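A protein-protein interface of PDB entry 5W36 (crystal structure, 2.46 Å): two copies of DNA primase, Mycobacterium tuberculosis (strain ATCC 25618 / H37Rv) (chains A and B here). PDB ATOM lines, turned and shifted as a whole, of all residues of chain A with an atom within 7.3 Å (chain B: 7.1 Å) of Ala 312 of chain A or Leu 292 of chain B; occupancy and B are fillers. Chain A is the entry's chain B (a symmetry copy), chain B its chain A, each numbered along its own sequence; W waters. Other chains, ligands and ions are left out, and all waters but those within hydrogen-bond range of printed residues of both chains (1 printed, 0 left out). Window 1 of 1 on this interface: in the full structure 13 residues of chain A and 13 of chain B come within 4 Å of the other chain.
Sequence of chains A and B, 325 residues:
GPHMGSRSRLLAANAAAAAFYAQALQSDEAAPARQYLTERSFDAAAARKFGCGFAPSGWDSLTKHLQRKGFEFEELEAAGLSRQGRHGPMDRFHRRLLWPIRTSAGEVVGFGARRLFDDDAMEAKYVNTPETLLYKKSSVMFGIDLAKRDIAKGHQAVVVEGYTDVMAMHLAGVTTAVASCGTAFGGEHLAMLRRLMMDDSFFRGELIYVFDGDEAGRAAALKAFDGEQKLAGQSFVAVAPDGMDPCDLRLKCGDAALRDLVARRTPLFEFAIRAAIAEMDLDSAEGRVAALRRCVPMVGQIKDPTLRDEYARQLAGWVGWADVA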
ATOM      1  N   ILE A 273       3.436 -10.287 -12.055  1.00  0.00           N
ATOM      2  CA  ILE A 273       2.860 -11.109 -10.981  1.00  0.00           C
ATOM      3  C   ILE A 273       2.991 -10.423  -9.629  1.00  0.00           C
ATOM      4  O   ILE A 273       2.003 -10.279  -8.908  1.00  0.00           O
ATOM      5  CB  ILE A 273       3.481 -12.522 -10.963  1.00  0.00           C
ATOM      6  CG1 ILE A 273       3.074 -13.277 -12.246  1.00  0.00           C
ATOM      7  CG2 ILE A 273       3.060 -13.310  -9.730  1.00  0.00           C
ATOM      8  CD1 ILE A 273       4.018 -14.396 -12.623  1.00  0.00           C
ATOM      9  N   LEU A 292      -3.499 -15.524  -4.286  1.00  0.00           N
ATOM     10  CA  LEU A 292      -3.278 -16.716  -5.125  1.00  0.00           C
ATOM     11  C   LEU A 292      -4.370 -16.898  -6.156  1.00  0.00           C
ATOM     12  O   LEU A 292      -4.100 -17.291  -7.280  1.00  0.00           O
ATOM     13  CB  LEU A 292      -3.161 -17.980  -4.286  1.00  0.00           C
ATOM     14  CG  LEU A 292      -1.839 -18.121  -3.554  1.00  0.00           C
ATOM     15  CD1 LEU A 292      -1.850 -19.406  -2.755  1.00  0.00           C
ATOM     16  CD2 LEU A 292      -0.654 -18.072  -4.512  1.00  0.00           C
ATOM     17  N   VAL A 296      -2.388 -17.140  -9.638  1.00  0.00           N
ATOM     18  CA  VAL A 296      -2.296 -18.485 -10.216  1.00  0.00           C
ATOM     19  C   VAL A 296      -2.833 -18.483 -11.654  1.00  0.00           C
ATOM     20  O   VAL A 296      -2.239 -19.118 -12.515  1.00  0.00           O
ATOM     21  CB  VAL A 296      -2.971 -19.580  -9.351  1.00  0.00           C
ATOM     22  CG1 VAL A 296      -2.992 -20.918 -10.083  1.00  0.00           C
ATOM     23  CG2 VAL A 296      -2.230 -19.748  -8.037  1.00  0.00           C
ATOM     24  N   VAL A 299       0.034 -17.143 -13.977  1.00  0.00           N
ATOM     25  CA  VAL A 299       0.987 -18.225 -14.252  1.00  0.00           C
ATOM     26  C   VAL A 299       0.379 -19.266 -15.194  1.00  0.00           C
ATOM     27  O   VAL A 299       1.075 -19.801 -16.053  1.00  0.00           O
ATOM     28  CB  VAL A 299       1.482 -18.881 -12.940  1.00  0.00           C
ATOM     29  CG1 VAL A 299       2.245 -20.166 -13.201  1.00  0.00           C
ATOM     30  CG2 VAL A 299       2.349 -17.898 -12.178  1.00  0.00           C
ATOM     31  N   ILE A 302       1.105 -18.543 -18.979  1.00  0.00           N
ATOM     32  CA  ILE A 302       2.470 -18.626 -19.503  1.00  0.00           C
ATOM     33  C   ILE A 302       2.587 -19.880 -20.361  1.00  0.00           C
ATOM     34  O   ILE A 302       2.447 -20.992 -19.864  1.00  0.00           O
ATOM     35  CB  ILE A 302       3.529 -18.619 -18.371  1.00  0.00           C
ATOM     36  CG1 ILE A 302       3.496 -17.268 -17.640  1.00  0.00           C
ATOM     37  CG2 ILE A 302       4.930 -18.890 -18.922  1.00  0.00           C
ATOM     38  CD1 ILE A 302       4.143 -17.258 -16.275  1.00  0.00           C
ATOM     39  N   THR A 306       8.593 -24.429 -19.110  1.00  0.00           N
ATOM     40  CA  THR A 306       9.744 -24.200 -18.223  1.00  0.00           C
ATOM     41  C   THR A 306       9.562 -22.938 -17.385  1.00  0.00           C
ATOM     42  O   THR A 306       9.773 -22.938 -16.178  1.00  0.00           O
ATOM     43  CB  THR A 306      11.052 -24.073 -19.026  1.00  0.00           C
ATOM     44  OG1 THR A 306      11.220 -25.241 -19.839  1.00  0.00           O
ATOM     45  CG2 THR A 306      12.276 -23.919 -18.094  1.00  0.00           C
ATOM     46  N   LEU A 307       9.143 -21.870 -18.046  1.00  0.00           N
ATOM     47  CA  LEU A 307       8.934 -20.582 -17.414  1.00  0.00           C
ATOM     48  C   LEU A 307       7.734 -20.612 -16.470  1.00  0.00           C
ATOM     49  O   LEU A 307       7.798 -20.075 -15.368  1.00  0.00           O
ATOM     50  CB  LEU A 307       8.741 -19.519 -18.500  1.00  0.00           C
ATOM     51  CG  LEU A 307       9.551 -18.235 -18.433  1.00  0.00           C
ATOM     52  CD1 LEU A 307      10.990 -18.448 -17.953  1.00  0.00           C
ATOM     53  CD2 LEU A 307       9.507 -17.606 -19.823  1.00  0.00           C
ATOM     54  N   ARG A 308       6.655 -21.268 -16.894  1.00  0.00           N
ATOM     55  CA  ARG A 308       5.477 -21.448 -16.046  1.00  0.00           C
ATOM     56  C   ARG A 308       5.837 -22.153 -14.753  1.00  0.00           C
ATOM     57  O   ARG A 308       5.472 -21.690 -13.674  1.00  0.00           O
ATOM     58  CB  ARG A 308       4.406 -22.246 -16.776  1.00  0.00           C
ATOM     59  CG  ARG A 308       3.071 -22.342 -16.060  1.00  0.00           C
ATOM     60  CD  ARG A 308       2.051 -23.058 -16.935  1.00  0.00           C
ATOM     61  NE  ARG A 308       2.504 -24.418 -17.218  1.00  0.00           N
ATOM     62  CZ  ARG A 308       2.118 -25.194 -18.237  1.00  0.00           C
ATOM     63  NH1 ARG A 308       1.228 -24.785 -19.131  1.00  0.00           N
ATOM     64  NH2 ARG A 308       2.646 -26.418 -18.355  1.00  0.00           N
ATOM     65  N   ASP A 309       6.565 -23.263 -14.858  1.00  0.00           N
ATOM     66  CA  ASP A 309       6.961 -24.006 -13.660  1.00  0.00           C
ATOM     67  C   ASP A 309       7.815 -23.154 -12.729  1.00  0.00           C
ATOM     68  O   ASP A 309       7.612 -23.180 -11.515  1.00  0.00           O
ATOM     69  CB  ASP A 309       7.716 -25.288 -14.002  1.00  0.00           C
ATOM     70  CG  ASP A 309       8.264 -25.980 -12.759  1.00  0.00           C
ATOM     71  OD1 ASP A 309       9.478 -26.281 -12.727  1.00  0.00           O
ATOM     72  OD2 ASP A 309       7.485 -26.182 -11.793  1.00  0.00           O
ATOM     73  N   GLU A 310       8.760 -22.411 -13.300  1.00  0.00           N
ATOM     74  CA  GLU A 310       9.620 -21.537 -12.521  1.00  0.00           C
ATOM     75  C   GLU A 310       8.829 -20.515 -11.687  1.00  0.00           C
ATOM     76  O   GLU A 310       9.182 -20.285 -10.533  1.00  0.00           O
ATOM     77  CB  GLU A 310      10.625 -20.840 -13.432  1.00  0.00           C
ATOM     78  CG  GLU A 310      11.504 -19.805 -12.748  1.00  0.00           C
ATOM     79  CD  GLU A 310      12.832 -19.591 -13.467  1.00  0.00           C
ATOM     80  OE1 GLU A 310      13.520 -20.599 -13.779  1.00  0.00           O
ATOM     81  OE2 GLU A 310      13.189 -18.412 -13.712  1.00  0.00           O
ATOM     82  N   TYR A 311       7.779 -19.917 -12.262  1.00  0.00           N
ATOM     83  CA  TYR A 311       6.930 -18.959 -11.526  1.00  0.00           C
ATOM     84  C   TYR A 311       5.969 -19.634 -10.563  1.00  0.00           C
ATOM     85  O   TYR A 311       5.722 -19.096  -9.496  1.00  0.00           O
ATOM     86  CB  TYR A 311       6.175 -17.996 -12.472  1.00  0.00           C
ATOM     87  CG  TYR A 311       7.124 -17.015 -13.093  1.00  0.00           C
ATOM     88  CD1 TYR A 311       7.677 -15.991 -12.335  1.00  0.00           C
ATOM     89  CD2 TYR A 311       7.522 -17.140 -14.411  1.00  0.00           C
ATOM     90  CE1 TYR A 311       8.581 -15.096 -12.885  1.00  0.00           C
ATOM     91  CE2 TYR A 311       8.424 -16.265 -14.974  1.00  0.00           C
ATOM     92  CZ  TYR A 311       8.954 -15.241 -14.211  1.00  0.00           C
ATOM     93  OH  TYR A 311       9.843 -14.374 -14.795  1.00  0.00           O
ATOM     94  N   ALA A 312       5.438 -20.795 -10.940  1.00  0.00           N
ATOM     95  CA  ALA A 312       4.571 -21.591 -10.057  1.00  0.00           C
ATOM     96  C   ALA A 312       5.276 -22.017  -8.779  1.00  0.00           C
ATOM     97  O   ALA A 312       4.662 -22.046  -7.714  1.00  0.00           O
ATOM     98  CB  ALA A 312       4.059 -22.821 -10.787  1.00  0.00           C
ATOM     99  N   ARG A 313       6.557 -22.362  -8.908  1.00  0.00           N
ATOM    100  CA  ARG A 313       7.420 -22.720  -7.780  1.00  0.00           C
ATOM    101  C   ARG A 313       7.509 -21.608  -6.728  1.00  0.00           C
ATOM    102  O   ARG A 313       7.500 -21.896  -5.536  1.00  0.00           O
ATOM    103  CB  ARG A 313       8.828 -23.070  -8.301  1.00  0.00           C
ATOM    104  CG  ARG A 313       9.884 -23.355  -7.236  1.00  0.00           C
ATOM    105  CD  ARG A 313      11.182 -23.871  -7.848  1.00  0.00           C
ATOM    106  NE  ARG A 313      11.726 -22.993  -8.895  1.00  0.00           N
ATOM    107  CZ  ARG A 313      12.389 -21.846  -8.694  1.00  0.00           C
ATOM    108  NH1 ARG A 313      12.831 -21.157  -9.746  1.00  0.00           N
ATOM    109  NH2 ARG A 313      12.611 -21.370  -7.466  1.00  0.00           N
ATOM    110  N   GLN A 314       7.583 -20.353  -7.177  1.00  0.00           N
ATOM    111  CA  GLN A 314       7.852 -19.199  -6.301  1.00  0.00           C
ATOM    112  C   GLN A 314       6.627 -18.473  -5.733  1.00  0.00           C
ATOM    113  O   GLN A 314       6.789 -17.573  -4.897  1.00  0.00           O
ATOM    114  CB  GLN A 314       8.672 -18.149  -7.058  1.00  0.00           C
ATOM    115  CG  GLN A 314      10.013 -18.617  -7.583  1.00  0.00           C
ATOM    116  CD  GLN A 314      10.694 -17.522  -8.362  1.00  0.00           C
ATOM    117  OE1 GLN A 314      11.325 -16.645  -7.780  1.00  0.00           O
ATOM    118  NE2 GLN A 314      10.544 -17.543  -9.684  1.00  0.00           N
ATOM    119  N   LEU A 315       5.423 -18.820  -6.187  1.00  0.00           N
ATOM    120  CA  LEU A 315       4.231 -18.050  -5.829  1.00  0.00           C
ATOM    121  C   LEU A 315       3.938 -18.057  -4.342  1.00  0.00           C
ATOM    122  O   LEU A 315       3.657 -17.006  -3.757  1.00  0.00           O
ATOM    123  CB  LEU A 315       2.985 -18.567  -6.550  1.00  0.00           C
ATOM    124  CG  LEU A 315       2.673 -18.059  -7.948  1.00  0.00           C
ATOM    125  CD1 LEU A 315       1.262 -18.527  -8.301  1.00  0.00           C
ATOM    126  CD2 LEU A 315       2.815 -16.540  -8.040  1.00  0.00           C
ATOM    127  N   ALA A 316       3.987 -19.244  -3.746  1.00  0.00           N
ATOM    128  CA  ALA A 316       3.688 -19.410  -2.328  1.00  0.00           C
ATOM    129  C   ALA A 316       4.642 -18.580  -1.483  1.00  0.00           C
ATOM    130  O   ALA A 316       4.211 -17.905  -0.554  1.00  0.00           O
ATOM    131  CB  ALA A 316       3.748 -20.878  -1.929  1.00  0.00           C
ATOM    132  N   GLY A 317       5.927 -18.623  -1.825  1.00  0.00           N
ATOM    133  CA  GLY A 317       6.928 -17.765  -1.206  1.00  0.00           C
ATOM    134  C   GLY A 317       6.634 -16.272  -1.289  1.00  0.00           C
ATOM    135  O   GLY A 317       6.881 -15.542  -0.330  1.00  0.00           O
ATOM    136  N   TRP A 318       6.101 -15.819  -2.425  1.00  0.00           N
ATOM    137  CA  TRP A 318       5.779 -14.398  -2.631  1.00  0.00           C
ATOM    138  C   TRP A 318       4.554 -13.901  -1.872  1.00  0.00           C
ATOM    139  O   TRP A 318       4.526 -12.743  -1.463  1.00  0.00           O
ATOM    140  CB  TRP A 318       5.604 -14.089  -4.114  1.00  0.00           C
ATOM    141  CG  TRP A 318       6.867 -14.208  -4.918  1.00  0.00           C
ATOM    142  CD1 TRP A 318       8.152 -14.198  -4.454  1.00  0.00           C
ATOM    143  CD2 TRP A 318       6.960 -14.296  -6.342  1.00  0.00           C
ATOM    144  NE1 TRP A 318       9.035 -14.296  -5.498  1.00  0.00           N
ATOM    145  CE2 TRP A 318       8.332 -14.353  -6.669  1.00  0.00           C
ATOM    146  CE3 TRP A 318       6.020 -14.330  -7.373  1.00  0.00           C
ATOM    147  CZ2 TRP A 318       8.784 -14.448  -7.983  1.00  0.00           C
ATOM    148  CZ3 TRP A 318       6.471 -14.433  -8.678  1.00  0.00           C
ATOM    149  CH2 TRP A 318       7.841 -14.490  -8.970  1.00  0.00           C
ATOM    150  N   ILE B 277      -4.272 -34.370  -6.776  1.00  0.00           N
ATOM    151  CA  ILE B 277      -4.044 -33.767  -5.447  1.00  0.00           C
ATOM    152  C   ILE B 277      -4.260 -34.769  -4.301  1.00  0.00           C
ATOM    153  O   ILE B 277      -3.556 -34.715  -3.300  1.00  0.00           O
ATOM    154  CB  ILE B 277      -4.919 -32.504  -5.233  1.00  0.00           C
ATOM    155  CG1 ILE B 277      -4.467 -31.390  -6.180  1.00  0.00           C
ATOM    156  CG2 ILE B 277      -4.870 -32.000  -3.784  1.00  0.00           C
ATOM    157  CD1 ILE B 277      -5.473 -30.278  -6.369  1.00  0.00           C
ATOM    158  N   MET B 280      -1.189 -36.698  -2.785  1.00  0.00           N
ATOM    159  CA  MET B 280      -0.074 -35.897  -2.280  1.00  0.00           C
ATOM    160  C   MET B 280      -0.306 -35.463  -0.832  1.00  0.00           C
ATOM    161  O   MET B 280      -1.449 -35.246  -0.417  1.00  0.00           O
ATOM    162  CB  MET B 280       0.131 -34.689  -3.194  1.00  0.00           C
ATOM    163  CG  MET B 280       0.439 -35.091  -4.632  1.00  0.00           C
ATOM    164  SD  MET B 280       0.908 -33.716  -5.689  1.00  0.00           S
ATOM    165  CE  MET B 280       2.598 -33.422  -5.170  1.00  0.00           C
ATOM    166  N   GLU B 286       5.540 -27.181   2.204  1.00  0.00           N
ATOM    167  CA  GLU B 286       6.295 -27.563   1.009  1.00  0.00           C
ATOM    168  C   GLU B 286       5.502 -28.574   0.163  1.00  0.00           C
ATOM    169  O   GLU B 286       5.629 -28.580  -1.069  1.00  0.00           O
ATOM    170  CB  GLU B 286       7.706 -28.089   1.356  1.00  0.00           C
ATOM    171  CG  GLU B 286       8.590 -27.145   2.197  1.00  0.00           C
ATOM    172  CD  GLU B 286       9.309 -26.039   1.418  1.00  0.00           C
ATOM    173  OE1 GLU B 286      10.525 -25.828   1.674  1.00  0.00           O
ATOM    174  OE2 GLU B 286       8.662 -25.358   0.584  1.00  0.00           O
ATOM    175  N   GLY B 287       4.673 -29.399   0.811  1.00  0.00           N
ATOM    176  CA  GLY B 287       3.733 -30.294   0.108  1.00  0.00           C
ATOM    177  C   GLY B 287       2.596 -29.555  -0.605  1.00  0.00           C
ATOM    178  O   GLY B 287       2.207 -29.906  -1.712  1.00  0.00           O
ATOM    179  N   ARG B 288       2.055 -28.530   0.038  1.00  0.00           N
ATOM    180  CA  ARG B 288       1.154 -27.591  -0.638  1.00  0.00           C
ATOM    181  C   ARG B 288       1.784 -27.036  -1.928  1.00  0.00           C
ATOM    182  O   ARG B 288       1.141 -27.029  -2.977  1.00  0.00           O
ATOM    183  CB  ARG B 288       0.761 -26.435   0.294  1.00  0.00           C
ATOM    184  CG  ARG B 288      -0.628 -26.529   0.917  1.00  0.00           C
ATOM    185  CD  ARG B 288      -0.665 -27.341   2.180  1.00  0.00           C
ATOM    186  NE  ARG B 288       0.016 -26.673   3.291  1.00  0.00           N
ATOM    187  CZ  ARG B 288      -0.484 -25.691   4.041  1.00  0.00           C
ATOM    188  NH1 ARG B 288      -1.712 -25.209   3.836  1.00  0.00           N
ATOM    189  NH2 ARG B 288       0.263 -25.182   5.020  1.00  0.00           N
ATOM    190  N   VAL B 289       3.040 -26.595  -1.846  1.00  0.00           N
ATOM    191  CA  VAL B 289       3.754 -26.033  -3.000  1.00  0.00           C
ATOM    192  C   VAL B 289       3.945 -27.099  -4.089  1.00  0.00           C
ATOM    193  O   VAL B 289       3.678 -26.838  -5.262  1.00  0.00           O
ATOM    194  CB  VAL B 289       5.125 -25.418  -2.591  1.00  0.00           C
ATOM    195  CG1 VAL B 289       5.983 -25.055  -3.809  1.00  0.00           C
ATOM    196  CG2 VAL B 289       4.921 -24.176  -1.727  1.00  0.00           C
ATOM    197  N   ALA B 290       4.389 -28.293  -3.695  1.00  0.00           N
ATOM    198  CA  ALA B 290       4.582 -29.400  -4.641  1.00  0.00           C
ATOM    199  C   ALA B 290       3.268 -29.787  -5.318  1.00  0.00           C
ATOM    200  O   ALA B 290       3.265 -30.157  -6.495  1.00  0.00           O
ATOM    201  CB  ALA B 290       5.199 -30.613  -3.946  1.00  0.00           C
ATOM    202  N   ALA B 291       2.164 -29.680  -4.574  1.00  0.00           N
ATOM    203  CA  ALA B 291       0.830 -29.963  -5.103  1.00  0.00           C
ATOM    204  C   ALA B 291       0.462 -28.946  -6.167  1.00  0.00           C
ATOM    205  O   ALA B 291       0.013 -29.316  -7.251  1.00  0.00           O
ATOM    206  CB  ALA B 291      -0.212 -29.983  -3.985  1.00  0.00           C
ATOM    207  N   LEU B 292       0.686 -27.674  -5.847  1.00  0.00           N
ATOM    208  CA  LEU B 292       0.503 -26.567  -6.790  1.00  0.00           C
ATOM    209  C   LEU B 292       1.355 -26.777  -8.039  1.00  0.00           C
ATOM    210  O   LEU B 292       0.880 -26.580  -9.148  1.00  0.00           O
ATOM    211  CB  LEU B 292       0.873 -25.224  -6.137  1.00  0.00           C
ATOM    212  CG  LEU B 292       0.136 -23.930  -6.504  1.00  0.00           C
ATOM    213  CD1 LEU B 292       1.046 -22.728  -6.269  1.00  0.00           C
ATOM    214  CD2 LEU B 292      -0.345 -23.904  -7.934  1.00  0.00           C
ATOM    215  N   ARG B 293       2.605 -27.194  -7.848  1.00  0.00           N
ATOM    216  CA  ARG B 293       3.507 -27.458  -8.967  1.00  0.00           C
ATOM    217  C   ARG B 293       3.081 -28.617  -9.861  1.00  0.00           C
ATOM    218  O   ARG B 293       3.382 -28.596 -11.044  1.00  0.00           O
ATOM    219  CB  ARG B 293       4.929 -27.708  -8.476  1.00  0.00           C
ATOM    220  CG  ARG B 293       5.618 -26.452  -7.979  1.00  0.00           C
ATOM    221  CD  ARG B 293       6.975 -26.285  -8.635  1.00  0.00           C
ATOM    222  NE  ARG B 293       8.053 -26.919  -7.886  1.00  0.00           N
ATOM    223  CZ  ARG B 293       9.284 -27.121  -8.350  1.00  0.00           C
ATOM    224  NH1 ARG B 293       9.627 -26.766  -9.585  1.00  0.00           N
ATOM    225  NH2 ARG B 293      10.188 -27.701  -7.566  1.00  0.00           N
ATOM    226  N   ARG B 294       2.409 -29.627  -9.313  1.00  0.00           N
ATOM    227  CA  ARG B 294       1.861 -30.710 -10.154  1.00  0.00           C
ATOM    228  C   ARG B 294       0.573 -30.315 -10.888  1.00  0.00           C
ATOM    229  O   ARG B 294       0.268 -30.874 -11.935  1.00  0.00           O
ATOM    230  CB  ARG B 294       1.645 -31.994  -9.337  1.00  0.00           C
ATOM    231  CG  ARG B 294       1.248 -33.216 -10.163  1.00  0.00           C
ATOM    232  CD  ARG B 294       1.864 -34.491  -9.603  1.00  0.00           C
ATOM    233  NE  ARG B 294       1.416 -35.702 -10.309  1.00  0.00           N
ATOM    234  CZ  ARG B 294       0.545 -36.615  -9.852  1.00  0.00           C
ATOM    235  NH1 ARG B 294      -0.047 -36.510  -8.656  1.00  0.00           N
ATOM    236  NH2 ARG B 294       0.252 -37.670 -10.618  1.00  0.00           N
ATOM    237  N   CYS B 295      -0.161 -29.340 -10.362  1.00  0.00           N
ATOM    238  CA  CYS B 295      -1.463 -28.963 -10.923  1.00  0.00           C
ATOM    239  C   CYS B 295      -1.439 -27.875 -11.996  1.00  0.00           C
ATOM    240  O   CYS B 295      -2.267 -27.936 -12.915  1.00  0.00           O
ATOM    241  CB  CYS B 295      -2.436 -28.585  -9.803  1.00  0.00           C
ATOM    242  SG  CYS B 295      -2.763 -29.999  -8.730  1.00  0.00           S
ATOM    243  N   VAL B 296      -0.526 -26.891 -11.916  1.00  0.00           N
ATOM    244  CA  VAL B 296      -0.501 -25.839 -12.965  1.00  0.00           C
ATOM    245  C   VAL B 296      -0.155 -26.378 -14.360  1.00  0.00           C
ATOM    246  O   VAL B 296      -0.699 -25.890 -15.343  1.00  0.00           O
ATOM    247  CB  VAL B 296       0.292 -24.541 -12.623  1.00  0.00           C
ATOM    248  CG1 VAL B 296      -0.038 -24.057 -11.224  1.00  0.00           C
ATOM    249  CG2 VAL B 296       1.792 -24.671 -12.797  1.00  0.00           C
ATOM    250  N   PRO B 297       0.714 -27.402 -14.454  1.00  0.00           N
ATOM    251  CA  PRO B 297       0.849 -28.073 -15.751  1.00  0.00           C
ATOM    252  C   PRO B 297      -0.452 -28.676 -16.287  1.00  0.00           C
ATOM    253  O   PRO B 297      -0.695 -28.600 -17.493  1.00  0.00           O
ATOM    254  CB  PRO B 297       1.868 -29.187 -15.466  1.00  0.00           C
ATOM    255  CG  PRO B 297       2.680 -28.648 -14.350  1.00  0.00           C
ATOM    256  CD  PRO B 297       1.694 -27.920 -13.489  1.00  0.00           C
ATOM    257  N   ALA B 312      -7.776 -22.594 -12.625  1.00  0.00           N
ATOM    258  CA  ALA B 312      -6.614 -21.940 -12.023  1.00  0.00           C
ATOM    259  C   ALA B 312      -6.966 -21.129 -10.771  1.00  0.00           C
ATOM    260  O   ALA B 312      -6.175 -21.063  -9.834  1.00  0.00           O
ATOM    261  CB  ALA B 312      -5.932 -21.050 -13.041  1.00  0.00           C
ATOM    262  N   LEU B 315      -7.421 -23.526  -7.671  1.00  0.00           N
ATOM    263  CA  LEU B 315      -6.308 -24.421  -7.340  1.00  0.00           C
ATOM    264  C   LEU B 315      -5.804 -24.230  -5.907  1.00  0.00           C
ATOM    265  O   LEU B 315      -5.505 -25.217  -5.232  1.00  0.00           O
ATOM    266  CB  LEU B 315      -5.150 -24.226  -8.333  1.00  0.00           C
ATOM    267  CG  LEU B 315      -4.577 -25.464  -9.010  1.00  0.00           C
ATOM    268  CD1 LEU B 315      -5.669 -26.275  -9.695  1.00  0.00           C
ATOM    269  CD2 LEU B 315      -3.524 -25.024 -10.016  1.00  0.00           C
ATOM    270  N   ALA B 316      -5.716 -22.975  -5.455  1.00  0.00           N
ATOM    271  CA  ALA B 316      -5.285 -22.645  -4.075  1.00  0.00           C
ATOM    272  C   ALA B 316      -6.154 -23.326  -3.025  1.00  0.00           C
ATOM    273  O   ALA B 316      -5.639 -23.980  -2.111  1.00  0.00           O
ATOM    274  CB  ALA B 316      -5.296 -21.142  -3.850  1.00  0.00           C
ATOM    275  N   VAL B 319      -5.729 -27.287  -2.920  1.00  0.00           N
ATOM    276  CA  VAL B 319      -4.458 -27.679  -2.326  1.00  0.00           C
ATOM    277  C   VAL B 319      -4.472 -27.447  -0.792  1.00  0.00           C
ATOM    278  O   VAL B 319      -3.600 -27.945  -0.086  1.00  0.00           O
ATOM    279  CB  VAL B 319      -3.312 -26.925  -3.066  1.00  0.00           C
ATOM    280  CG1 VAL B 319      -2.033 -26.841  -2.266  1.00  0.00           C
ATOM    281  CG2 VAL B 319      -3.038 -27.585  -4.409  1.00  0.00           C
ATOM    282  N   ALA B 322      -2.464 -23.465  -0.131  1.00  0.00           N
ATOM    283  CA  ALA B 322      -1.057 -23.370  -0.612  1.00  0.00           C
ATOM    284  C   ALA B 322      -0.066 -22.799   0.400  1.00  0.00           C
ATOM    285  O   ALA B 322      -0.403 -22.615   1.566  1.00  0.00           O
ATOM    286  CB  ALA B 322      -0.973 -22.609  -1.925  1.00  0.00           C
HETATM  287  O   HOH W   1       4.823 -26.221 -11.891  1.00  0.00           O
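NH1 of Arg 293 of chain B lies within salt-bridge range of OD2 of Asp 309 of chain A (3.1 Å).
Among the printed residues, pairs that only touch across the chains: Leu 292 of chain A with Ala 316 of chain B (3.8 Å), Leu 292 of chain A with Ala 322 of chain B (3.4 Å), Val 296 of chain A with Ala 312 of chain B (3.2 Å), Arg 308 of chain A with Val 296 of chain B (3.99 Å), Arg 308 of chain A with Pro 297 of chain B (3.6 Å), Ala 312 of chain A with Leu 292 of chain B (3.95 Å), Ala 312 of chain A with Val 296 of chain B (3.5 Å), Arg 313 of chain A with Val 289 of chain B (3.9 Å), Arg 313 of chain A with Arg 293 of chain B (3.7 Å) and Ala 316 of chain A with Val 289 of chain B (3.5 Å).
Ala 312 of chain A touches just these residues of chain B: Leu 292 (3.95 Å) and Val 296 (3.5 Å). Leu 292 of chain B touches just one residue of chain A: Ala 312 (3.95 Å). No residue of chain A comes within 4 Å of Ala 291 of chain B. Printed residues of chain A within 4 Å of Pro 297 of chain B: Arg 308 (3.6 Å). Of the printed residues of chain B, Val 296 of chain A touches Ala 312 (3.2 Å). Ile 273 of chain A touches none of the printed residues of chain B. Met 280 of chain B touches none of the printed residues of chain A. The nearest residue of chain A that does not touch Leu 292 of chain B is Val 296 of chain A (4.5 Å).
Of the 19 printed residues of chain B, 8 touch a printed residue of chain A. Printed residues of chain B that touch a printed residue of chain A: Val 289, Leu 292, Arg 293, Val 296, Pro 297, Ala 312, Ala 316 and Ala 322. Among the printed residues, Asp or Glu carboxylates within 4 Å of a Lys or Arg side-chain nitrogen of the other chain: Asp 309 of chain A with Arg 293 of chain B.
Leu 292 of chain A touches Ala 316 of chain B, but with the chains exchanged Ala 316 of chain A does not touch Leu 292 of chain B (5.2 Å). Val 296 of chain A touches Ala 312 of chain B, and with the chains exchanged Ala 312 of chain A touches Val 296 of chain B. Ala 312 of chain A touches Leu 292 of chain B, but with the chains exchanged Leu 292 of chain A does not touch Ala 312 of chain B (5.0 Å). Positions printed for both chains: 292, 296, 312, 315 and 316.
Water W1 lies within hydrogen-bond range of OD2 of Asp 309 of chain A and O of Arg 293 of chain B.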
